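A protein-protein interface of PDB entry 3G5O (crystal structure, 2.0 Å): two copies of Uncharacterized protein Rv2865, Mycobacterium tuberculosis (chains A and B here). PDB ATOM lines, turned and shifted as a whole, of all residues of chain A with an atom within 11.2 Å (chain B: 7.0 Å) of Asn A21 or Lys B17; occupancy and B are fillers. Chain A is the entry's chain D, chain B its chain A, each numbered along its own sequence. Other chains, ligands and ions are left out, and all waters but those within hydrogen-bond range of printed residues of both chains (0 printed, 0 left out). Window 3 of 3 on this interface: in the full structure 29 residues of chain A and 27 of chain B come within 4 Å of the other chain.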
ATOM      1  N   ARG A   9      -3.388 -30.787  29.176  1.00  0.00           N
ATOM      2  CA  ARG A   9      -4.152 -29.576  29.041  1.00  0.00           C
ATOM      3  C   ARG A   9      -4.279 -29.242  27.561  1.00  0.00           C
ATOM      4  O   ARG A   9      -3.378 -29.508  26.772  1.00  0.00           O
ATOM      5  CB  ARG A   9      -3.441 -28.435  29.740  1.00  0.00           C
ATOM      6  CG  ARG A   9      -3.651 -28.388  31.232  1.00  0.00           C
ATOM      7  CD  ARG A   9      -3.369 -26.971  31.713  1.00  0.00           C
ATOM      8  NE  ARG A   9      -1.933 -26.700  31.766  1.00  0.00           N
ATOM      9  CZ  ARG A   9      -1.427 -25.488  31.994  1.00  0.00           C
ATOM     10  NH1 ARG A   9      -2.250 -24.441  32.167  1.00  0.00           N
ATOM     11  NH2 ARG A   9      -0.112 -25.313  32.040  1.00  0.00           N
ATOM     12  N   ILE A  13      -3.712 -21.486  20.920  1.00  0.00           N
ATOM     13  CA  ILE A  13      -2.408 -20.832  20.696  1.00  0.00           C
ATOM     14  C   ILE A  13      -2.407 -19.371  21.192  1.00  0.00           C
ATOM     15  O   ILE A  13      -1.372 -18.872  21.641  1.00  0.00           O
ATOM     16  CB  ILE A  13      -1.867 -20.951  19.240  1.00  0.00           C
ATOM     17  CG1 ILE A  13      -0.371 -20.539  19.191  1.00  0.00           C
ATOM     18  CG2 ILE A  13      -2.723 -20.144  18.244  1.00  0.00           C
ATOM     19  CD1 ILE A  13       0.303 -20.874  17.862  1.00  0.00           C
ATOM     20  N   THR A  15      -3.444 -18.279  23.870  1.00  0.00           N
ATOM     21  CA  THR A  15      -3.029 -18.346  25.276  1.00  0.00           C
ATOM     22  C   THR A  15      -1.510 -18.537  25.450  1.00  0.00           C
ATOM     23  O   THR A  15      -0.904 -18.044  26.399  1.00  0.00           O
ATOM     24  CB  THR A  15      -3.836 -19.471  26.016  1.00  0.00           C
ATOM     25  OG1 THR A  15      -5.207 -19.097  26.033  1.00  0.00           O
ATOM     26  CG2 THR A  15      -3.385 -19.657  27.470  1.00  0.00           C
ATOM     27  N   ILE A  16      -0.888 -19.264  24.536  1.00  0.00           N
ATOM     28  CA  ILE A  16       0.564 -19.517  24.611  1.00  0.00           C
ATOM     29  C   ILE A  16       1.401 -18.282  24.186  1.00  0.00           C
ATOM     30  O   ILE A  16       2.456 -18.012  24.775  1.00  0.00           O
ATOM     31  CB  ILE A  16       0.983 -20.735  23.729  1.00  0.00           C
ATOM     32  CG1 ILE A  16       0.113 -21.964  24.025  1.00  0.00           C
ATOM     33  CG2 ILE A  16       2.433 -21.100  23.959  1.00  0.00           C
ATOM     34  CD1 ILE A  16       0.043 -22.323  25.508  1.00  0.00           C
ATOM     35  N   LYS A  17       0.922 -17.544  23.184  1.00  0.00           N
ATOM     36  CA  LYS A  17       1.703 -16.436  22.599  1.00  0.00           C
ATOM     37  C   LYS A  17       2.184 -15.445  23.652  1.00  0.00           C
ATOM     38  O   LYS A  17       1.407 -15.036  24.522  1.00  0.00           O
ATOM     39  CB  LYS A  17       0.874 -15.660  21.589  1.00  0.00           C
ATOM     40  CG  LYS A  17       0.826 -16.237  20.218  1.00  0.00           C
ATOM     41  CD  LYS A  17       0.357 -15.145  19.269  1.00  0.00           C
ATOM     42  CE  LYS A  17      -0.886 -15.557  18.499  1.00  0.00           C
ATOM     43  NZ  LYS A  17      -0.526 -16.490  17.419  1.00  0.00           N
ATOM     44  N   GLY A  18       3.455 -15.064  23.562  1.00  0.00           N
ATOM     45  CA  GLY A  18       4.039 -14.103  24.508  1.00  0.00           C
ATOM     46  C   GLY A  18       4.279 -14.681  25.898  1.00  0.00           C
ATOM     47  O   GLY A  18       4.748 -13.967  26.805  1.00  0.00           O
ATOM     48  N   LYS A  19       3.943 -15.960  26.086  1.00  0.00           N
ATOM     49  CA  LYS A  19       4.031 -16.597  27.407  1.00  0.00           C
ATOM     50  C   LYS A  19       4.766 -17.939  27.328  1.00  0.00           C
ATOM     51  O   LYS A  19       4.584 -18.826  28.162  1.00  0.00           O
ATOM     52  CB  LYS A  19       2.634 -16.774  28.016  1.00  0.00           C
ATOM     53  CG  LYS A  19       1.876 -15.447  28.314  1.00  0.00           C
ATOM     54  CD  LYS A  19       1.068 -15.543  29.609  1.00  0.00           C
ATOM     55  CE  LYS A  19       0.163 -14.316  29.865  1.00  0.00           C
ATOM     56  NZ  LYS A  19      -0.711 -13.940  28.698  1.00  0.00           N
ATOM     57  N   LEU A  20       5.622 -18.063  26.333  1.00  0.00           N
ATOM     58  CA  LEU A  20       6.215 -19.344  26.013  1.00  0.00           C
ATOM     59  C   LEU A  20       7.227 -19.770  27.091  1.00  0.00           C
ATOM     60  O   LEU A  20       7.300 -20.952  27.413  1.00  0.00           O
ATOM     61  CB  LEU A  20       6.829 -19.293  24.618  1.00  0.00           C
ATOM     62  CG  LEU A  20       7.275 -20.633  24.037  1.00  0.00           C
ATOM     63  CD1 LEU A  20       6.110 -21.644  23.915  1.00  0.00           C
ATOM     64  CD2 LEU A  20       7.938 -20.371  22.688  1.00  0.00           C
ATOM     65  N   ASN A  21       7.958 -18.809  27.678  1.00  0.00           N
ATOM     66  CA  ASN A  21       8.817 -19.099  28.849  1.00  0.00           C
ATOM     67  C   ASN A  21       8.070 -19.853  29.936  1.00  0.00           C
ATOM     68  O   ASN A  21       8.561 -20.851  30.456  1.00  0.00           O
ATOM     69  CB  ASN A  21       9.396 -17.837  29.502  1.00  0.00           C
ATOM     70  CG  ASN A  21      10.483 -17.194  28.677  1.00  0.00           C
ATOM     71  OD1 ASN A  21      10.408 -16.005  28.387  1.00  0.00           O
ATOM     72  ND2 ASN A  21      11.496 -17.957  28.300  1.00  0.00           N
ATOM     73  N   GLU A  22       6.892 -19.351  30.287  1.00  0.00           N
ATOM     74  CA  GLU A  22       6.143 -19.924  31.385  1.00  0.00           C
ATOM     75  C   GLU A  22       5.616 -21.317  31.001  1.00  0.00           C
ATOM     76  O   GLU A  22       5.657 -22.216  31.824  1.00  0.00           O
ATOM     77  CB  GLU A  22       5.050 -18.973  31.914  1.00  0.00           C
ATOM     78  CG  GLU A  22       3.598 -19.263  31.455  1.00  0.00           C
ATOM     79  CD  GLU A  22       2.503 -18.684  32.397  1.00  0.00           C
ATOM     80  OE1 GLU A  22       1.691 -17.836  31.934  1.00  0.00           O
ATOM     81  OE2 GLU A  22       2.443 -19.080  33.594  1.00  0.00           O
ATOM     82  N   PHE A  23       5.187 -21.517  29.753  1.00  0.00           N
ATOM     83  CA  PHE A  23       4.693 -22.818  29.384  1.00  0.00           C
ATOM     84  C   PHE A  23       5.782 -23.863  29.230  1.00  0.00           C
ATOM     85  O   PHE A  23       5.552 -25.013  29.596  1.00  0.00           O
ATOM     86  CB  PHE A  23       3.729 -22.763  28.198  1.00  0.00           C
ATOM     87  CG  PHE A  23       2.411 -22.169  28.557  1.00  0.00           C
ATOM     88  CD1 PHE A  23       1.496 -22.899  29.328  1.00  0.00           C
ATOM     89  CD2 PHE A  23       2.098 -20.866  28.187  1.00  0.00           C
ATOM     90  CE1 PHE A  23       0.253 -22.341  29.700  1.00  0.00           C
ATOM     91  CE2 PHE A  23       0.858 -20.280  28.547  1.00  0.00           C
ATOM     92  CZ  PHE A  23      -0.071 -21.020  29.301  1.00  0.00           C
ATOM     93  N   VAL A  24       6.942 -23.467  28.706  1.00  0.00           N
ATOM     94  CA  VAL A  24       8.104 -24.347  28.671  1.00  0.00           C
ATOM     95  C   VAL A  24       8.530 -24.719  30.111  1.00  0.00           C
ATOM     96  O   VAL A  24       8.813 -25.910  30.395  1.00  0.00           O
ATOM     97  CB  VAL A  24       9.259 -23.706  27.869  1.00  0.00           C
ATOM     98  CG1 VAL A  24      10.600 -24.379  28.148  1.00  0.00           C
ATOM     99  CG2 VAL A  24       8.924 -23.744  26.361  1.00  0.00           C
ATOM    100  N   ASP A  25       8.540 -23.733  31.017  1.00  0.00           N
ATOM    101  CA  ASP A  25       8.844 -24.022  32.426  1.00  0.00           C
ATOM    102  C   ASP A  25       7.819 -24.999  32.993  1.00  0.00           C
ATOM    103  O   ASP A  25       8.201 -25.934  33.683  1.00  0.00           O
ATOM    104  CB  ASP A  25       8.869 -22.760  33.311  1.00  0.00           C
ATOM    105  CG  ASP A  25      10.121 -21.930  33.136  1.00  0.00           C
ATOM    106  OD1 ASP A  25      11.123 -22.420  32.561  1.00  0.00           O
ATOM    107  OD2 ASP A  25      10.095 -20.740  33.569  1.00  0.00           O
ATOM    108  N   ALA A  26       6.538 -24.805  32.681  1.00  0.00           N
ATOM    109  CA  ALA A  26       5.488 -25.681  33.213  1.00  0.00           C
ATOM    110  C   ALA A  26       5.600 -27.157  32.782  1.00  0.00           C
ATOM    111  O   ALA A  26       5.180 -28.054  33.543  1.00  0.00           O
ATOM    112  CB  ALA A  26       4.113 -25.136  32.890  1.00  0.00           C
ATOM    113  N   VAL A  27       6.154 -27.417  31.590  1.00  0.00           N
ATOM    114  CA  VAL A  27       6.298 -28.812  31.123  1.00  0.00           C
ATOM    115  C   VAL A  27       7.670 -29.410  31.390  1.00  0.00           C
ATOM    116  O   VAL A  27       7.758 -30.606  31.584  1.00  0.00           O
ATOM    117  CB  VAL A  27       5.906 -29.049  29.629  1.00  0.00           C
ATOM    118  CG1 VAL A  27       4.449 -28.700  29.389  1.00  0.00           C
ATOM    119  CG2 VAL A  27       6.833 -28.270  28.648  1.00  0.00           C
ATOM    120  N   SER A  28       8.724 -28.597  31.433  1.00  0.00           N
ATOM    121  CA  SER A  28      10.080 -29.149  31.575  1.00  0.00           C
ATOM    122  C   SER A  28      10.263 -29.819  32.939  1.00  0.00           C
ATOM    123  O   SER A  28      11.075 -30.736  33.105  1.00  0.00           O
ATOM    124  CB  SER A  28      11.172 -28.100  31.343  1.00  0.00           C
ATOM    125  OG  SER A  28      11.175 -27.113  32.339  1.00  0.00           O
ATOM    126  N   SER A  29       9.470 -29.374  33.897  1.00  0.00           N
ATOM    127  CA  SER A  29       9.649 -29.827  35.251  1.00  0.00           C
ATOM    128  C   SER A  29       8.672 -30.944  35.618  1.00  0.00           C
ATOM    129  O   SER A  29       8.745 -31.466  36.724  1.00  0.00           O
ATOM    130  CB  SER A  29       9.577 -28.639  36.242  1.00  0.00           C
ATOM    131  OG  SER A  29       8.434 -27.806  36.050  1.00  0.00           O
ATOM    132  N   ILE A  34       0.814 -30.288  26.944  1.00  0.00           N
ATOM    133  CA  ILE A  34      -0.066 -29.258  26.461  1.00  0.00           C
ATOM    134  C   ILE A  34      -0.341 -29.518  24.998  1.00  0.00           C
ATOM    135  O   ILE A  34       0.580 -29.581  24.182  1.00  0.00           O
ATOM    136  CB  ILE A  34       0.511 -27.856  26.648  1.00  0.00           C
ATOM    137  CG1 ILE A  34       0.662 -27.566  28.151  1.00  0.00           C
ATOM    138  CG2 ILE A  34      -0.399 -26.788  25.972  1.00  0.00           C
ATOM    139  CD1 ILE A  34       1.680 -26.492  28.415  1.00  0.00           C
ATOM    140  N   ILE A  36      -1.766 -27.742  21.874  1.00  0.00           N
ATOM    141  CA  ILE A  36      -2.050 -26.373  21.440  1.00  0.00           C
ATOM    142  C   ILE A  36      -3.016 -26.406  20.272  1.00  0.00           C
ATOM    143  O   ILE A  36      -2.764 -27.106  19.287  1.00  0.00           O
ATOM    144  CB  ILE A  36      -0.753 -25.684  20.996  1.00  0.00           C
ATOM    145  CG1 ILE A  36       0.230 -25.628  22.183  1.00  0.00           C
ATOM    146  CG2 ILE A  36      -1.073 -24.265  20.517  1.00  0.00           C
ATOM    147  CD1 ILE A  36       1.654 -25.264  21.801  1.00  0.00           C
ATOM    148  N   LEU A  46       3.214 -29.894  23.223  1.00  0.00           N
ATOM    149  CA  LEU A  46       4.413 -29.511  23.960  1.00  0.00           C
ATOM    150  C   LEU A  46       4.620 -30.406  25.215  1.00  0.00           C
ATOM    151  O   LEU A  46       3.715 -30.537  26.029  1.00  0.00           O
ATOM    152  CB  LEU A  46       4.288 -28.043  24.401  1.00  0.00           C
ATOM    153  CG  LEU A  46       5.491 -27.325  25.076  1.00  0.00           C
ATOM    154  CD1 LEU A  46       6.638 -27.075  24.078  1.00  0.00           C
ATOM    155  CD2 LEU A  46       5.110 -25.967  25.726  1.00  0.00           C
ATOM    156  N   VAL A  47       5.803 -31.003  25.369  1.00  0.00           N
ATOM    157  CA  VAL A  47       6.127 -31.746  26.593  1.00  0.00           C
ATOM    158  C   VAL A  47       7.531 -31.394  27.050  1.00  0.00           C
ATOM    159  O   VAL A  47       8.322 -30.864  26.292  1.00  0.00           O
ATOM    160  CB  VAL A  47       6.061 -33.304  26.386  1.00  0.00           C
ATOM    161  CG1 VAL A  47       4.658 -33.723  26.010  1.00  0.00           C
ATOM    162  CG2 VAL A  47       7.056 -33.763  25.324  1.00  0.00           C
ATOM    163  N   GLY A  48       7.850 -31.730  28.296  1.00  0.00           N
ATOM    164  CA  GLY A  48       9.184 -31.527  28.804  1.00  0.00           C
ATOM    165  C   GLY A  48      10.198 -32.382  28.047  1.00  0.00           C
ATOM    166  O   GLY A  48       9.854 -33.434  27.508  1.00  0.00           O
ATOM    167  N   PRO B  12      16.750 -22.256  20.249  1.00  0.00           N
ATOM    168  CA  PRO B  12      16.517 -21.456  21.452  1.00  0.00           C
ATOM    169  C   PRO B  12      15.108 -20.886  21.462  1.00  0.00           C
ATOM    170  O   PRO B  12      14.530 -20.667  20.409  1.00  0.00           O
ATOM    171  CB  PRO B  12      17.558 -20.323  21.350  1.00  0.00           C
ATOM    172  CG  PRO B  12      17.994 -20.300  19.902  1.00  0.00           C
ATOM    173  CD  PRO B  12      17.793 -21.681  19.359  1.00  0.00           C
ATOM    174  N   ILE B  13      14.581 -20.648  22.656  1.00  0.00           N
ATOM    175  CA  ILE B  13      13.255 -20.117  22.835  1.00  0.00           C
ATOM    176  C   ILE B  13      13.109 -18.739  22.169  1.00  0.00           C
ATOM    177  O   ILE B  13      12.042 -18.430  21.627  1.00  0.00           O
ATOM    178  CB  ILE B  13      12.906 -20.094  24.346  1.00  0.00           C
ATOM    179  CG1 ILE B  13      11.430 -20.371  24.594  1.00  0.00           C
ATOM    180  CG2 ILE B  13      13.386 -18.802  25.024  1.00  0.00           C
ATOM    181  CD1 ILE B  13      11.108 -20.556  26.093  1.00  0.00           C
ATOM    182  N   SER B  14      14.193 -17.940  22.167  1.00  0.00           N
ATOM    183  CA  SER B  14      14.220 -16.638  21.470  1.00  0.00           C
ATOM    184  C   SER B  14      13.947 -16.746  19.967  1.00  0.00           C
ATOM    185  O   SER B  14      13.344 -15.856  19.388  1.00  0.00           O
ATOM    186  CB  SER B  14      15.544 -15.893  21.709  1.00  0.00           C
ATOM    187  OG  SER B  14      16.648 -16.626  21.191  1.00  0.00           O
ATOM    188  N   THR B  15      14.373 -17.835  19.343  1.00  0.00           N
ATOM    189  CA  THR B  15      14.092 -18.052  17.940  1.00  0.00           C
ATOM    190  C   THR B  15      12.612 -18.373  17.736  1.00  0.00           C
ATOM    191  O   THR B  15      12.031 -17.992  16.713  1.00  0.00           O
ATOM    192  CB  THR B  15      14.994 -19.162  17.373  1.00  0.00           C
ATOM    193  OG1 THR B  15      16.370 -18.801  17.567  1.00  0.00           O
ATOM    194  CG2 THR B  15      14.736 -19.398  15.881  1.00  0.00           C
ATOM    195  N   ILE B  16      11.999 -19.064  18.707  1.00  0.00           N
ATOM    196  CA  ILE B  16      10.577 -19.419  18.599  1.00  0.00           C
ATOM    197  C   ILE B  16       9.643 -18.213  18.805  1.00  0.00           C
ATOM    198  O   ILE B  16       8.703 -18.015  18.040  1.00  0.00           O
ATOM    199  CB  ILE B  16      10.164 -20.599  19.537  1.00  0.00           C
ATOM    200  CG1 ILE B  16      11.126 -21.797  19.411  1.00  0.00           C
ATOM    201  CG2 ILE B  16       8.722 -21.044  19.261  1.00  0.00           C
ATOM    202  CD1 ILE B  16      11.119 -22.480  18.070  1.00  0.00           C
ATOM    203  N   LYS B  17       9.915 -17.422  19.838  1.00  0.00           N
ATOM    204  CA  LYS B  17       9.066 -16.290  20.235  1.00  0.00           C
ATOM    205  C   LYS B  17       8.780 -15.334  19.077  1.00  0.00           C
ATOM    206  O   LYS B  17       9.699 -14.827  18.433  1.00  0.00           O
ATOM    207  CB  LYS B  17       9.716 -15.492  21.375  1.00  0.00           C
ATOM    208  CG  LYS B  17       9.942 -16.237  22.711  1.00  0.00           C
ATOM    209  CD  LYS B  17      10.071 -15.227  23.868  1.00  0.00           C
ATOM    210  CE  LYS B  17      10.939 -15.748  25.014  1.00  0.00           C
ATOM    211  NZ  LYS B  17      12.403 -15.511  24.783  1.00  0.00           N
ATOM    212  N   GLY B  18       7.502 -15.083  18.823  1.00  0.00           N
ATOM    213  CA  GLY B  18       7.106 -14.157  17.754  1.00  0.00           C
ATOM    214  C   GLY B  18       6.798 -14.846  16.435  1.00  0.00           C
ATOM    215  O   GLY B  18       6.065 -14.279  15.596  1.00  0.00           O
ATOM    216  N   LYS B  19       7.371 -16.052  16.247  1.00  0.00           N
ATOM    217  CA  LYS B  19       7.038 -16.927  15.121  1.00  0.00           C
ATOM    218  C   LYS B  19       6.261 -18.194  15.580  1.00  0.00           C
ATOM    219  O   LYS B  19       6.301 -19.240  14.929  1.00  0.00           O
ATOM    220  CB  LYS B  19       8.283 -17.276  14.270  1.00  0.00           C
ATOM    221  CG  LYS B  19       8.741 -16.151  13.269  1.00  0.00           C
ATOM    222  CD  LYS B  19       9.029 -16.721  11.867  1.00  0.00           C
ATOM    223  CE  LYS B  19       9.135 -15.628  10.788  1.00  0.00           C
ATOM    224  NZ  LYS B  19      10.554 -15.215  10.522  1.00  0.00           N
ATOM    225  N   LEU B  20       5.528 -18.070  16.680  1.00  0.00           N
ATOM    226  CA  LEU B  20       4.887 -19.235  17.289  1.00  0.00           C
ATOM    227  C   LEU B  20       3.922 -19.873  16.303  1.00  0.00           C
ATOM    228  O   LEU B  20       3.903 -21.094  16.160  1.00  0.00           O
ATOM    229  CB  LEU B  20       4.141 -18.864  18.580  1.00  0.00           C
ATOM    230  CG  LEU B  20       4.197 -19.815  19.792  1.00  0.00           C
ATOM    231  CD1 LEU B  20       2.854 -19.840  20.503  1.00  0.00           C
ATOM    232  CD2 LEU B  20       4.700 -21.247  19.565  1.00  0.00           C
ATOM    233  N   PHE B  23       5.940 -21.948  13.671  1.00  0.00           N
ATOM    234  CA  PHE B  23       6.530 -23.190  14.205  1.00  0.00           C
ATOM    235  C   PHE B  23       5.459 -24.242  14.507  1.00  0.00           C
ATOM    236  O   PHE B  23       5.670 -25.431  14.225  1.00  0.00           O
ATOM    237  CB  PHE B  23       7.434 -22.922  15.429  1.00  0.00           C
ATOM    238  CG  PHE B  23       8.798 -22.400  15.048  1.00  0.00           C
ATOM    239  CD1 PHE B  23       9.755 -23.254  14.501  1.00  0.00           C
ATOM    240  CD2 PHE B  23       9.117 -21.046  15.196  1.00  0.00           C
ATOM    241  CE1 PHE B  23      11.021 -22.775  14.121  1.00  0.00           C
ATOM    242  CE2 PHE B  23      10.372 -20.558  14.821  1.00  0.00           C
ATOM    243  CZ  PHE B  23      11.338 -21.433  14.275  1.00  0.00           C
ATOM    244  N   LYS B  38      16.559 -23.671  26.740  1.00  0.00           N
ATOM    245  CA  LYS B  38      16.457 -22.570  27.677  1.00  0.00           C
ATOM    246  C   LYS B  38      17.776 -22.629  28.439  1.00  0.00           C
ATOM    247  O   LYS B  38      18.133 -23.683  28.980  1.00  0.00           O
ATOM    248  CB  LYS B  38      15.285 -22.792  28.626  1.00  0.00           C
ATOM    249  CG  LYS B  38      14.454 -21.558  28.917  1.00  0.00           C
ATOM    250  CD  LYS B  38      13.607 -21.741  30.170  1.00  0.00           C
ATOM    251  CE  LYS B  38      13.039 -20.397  30.628  1.00  0.00           C
ATOM    252  NZ  LYS B  38      12.840 -20.306  32.119  1.00  0.00           N
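The side-chain hydroxyl (OG) of Ser A28 lies within hydrogen-bond range of the backbone carbonyl oxygen (O) of Val A24, at 3.3 Å. The backbone carbonyl oxygen (O) of Asp A25 sits at hydrogen-bond distance from the side-chain hydroxyl (OG) of Ser A29 (3.0 Å). The backbone carbonyl oxygen (O) of Asp A25 is in hydrogen-bond range of the side-chain hydroxyl (OG) of Ser A28 (3.5 Å).
Of chain A, only Asn A21 comes within 4 Å of Lys B17. Ile B13 touches just these residues of chain A: Leu A20 (3.98 Å), Asn A21 (3.4 Å) and Val A24 (3.9 Å). No residue of chain A comes within 4 Å of Thr B15. Printed residues of chain A within 4 Å of Ile B16: Leu A20. Printed residues of chain B within 4 Å of Leu A20: Ile B13 and Ile B16. Printed residues of chain A within 4 Å of Lys B38: Asn A21 and Asp A25. Of the printed residues of chain B, Ile A16 touches Leu B20. Of the printed residues of chain A, Leu B20 touches Ile A13 (3.6 Å) and Ile A16 (3.7 Å). Of the printed residues of chain B, Val A24 touches Ile B13 (3.9 Å). Lys A17 touches none of the printed residues of chain B. Gly A18 touches none of the printed residues of chain B. The nearest residue of chain A that does not touch Lys B17 is Leu A20 (4.6 Å).
CG1 of Ile A13 touches CD1 of Leu B20, at 3.6 Å. Ile A16 touches Leu B20 (CG2 to CD1, 3.7 Å). Ile B13 touches Leu A20. Ile B16 touches Leu A20 (CG2 to CD2, 3.6 Å). ND2 of Asn A21 touches CD1 of Ile B13, 3.4 Å away. Lys B17 touches Asn A21. Asn A21 touches Lys B38 (ND2 to CE, 3.7 Å). Val A24 touches Ile B13.
Ile A13 touches Leu B20, and with the chains exchanged Leu A20 touches Ile B13. Ile A16 touches Leu B20, and with the chains exchanged Leu A20 touches Ile B16. 8 positions are printed for both chains.
NZ of Lys B38 lies within salt-bridge range of OD1 of Asp A25.
Hydrophobic or aromatic side chains of chain B within 4 Å of the printed part of chain A: Ile B13, Ile B16 and Leu B20. Of the 22 printed residues of chain A, 6 touch a printed residue of chain B. Hydrophobic or aromatic side chains of chain A that line the printed part of chain B: Ile A13, Ile A16, Leu A20 and Val A24. Among the printed residues, Asp or Glu carboxylates within 4 Å of a Lys or Arg side-chain nitrogen of the other chain: Asp A25 with Lys B38.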
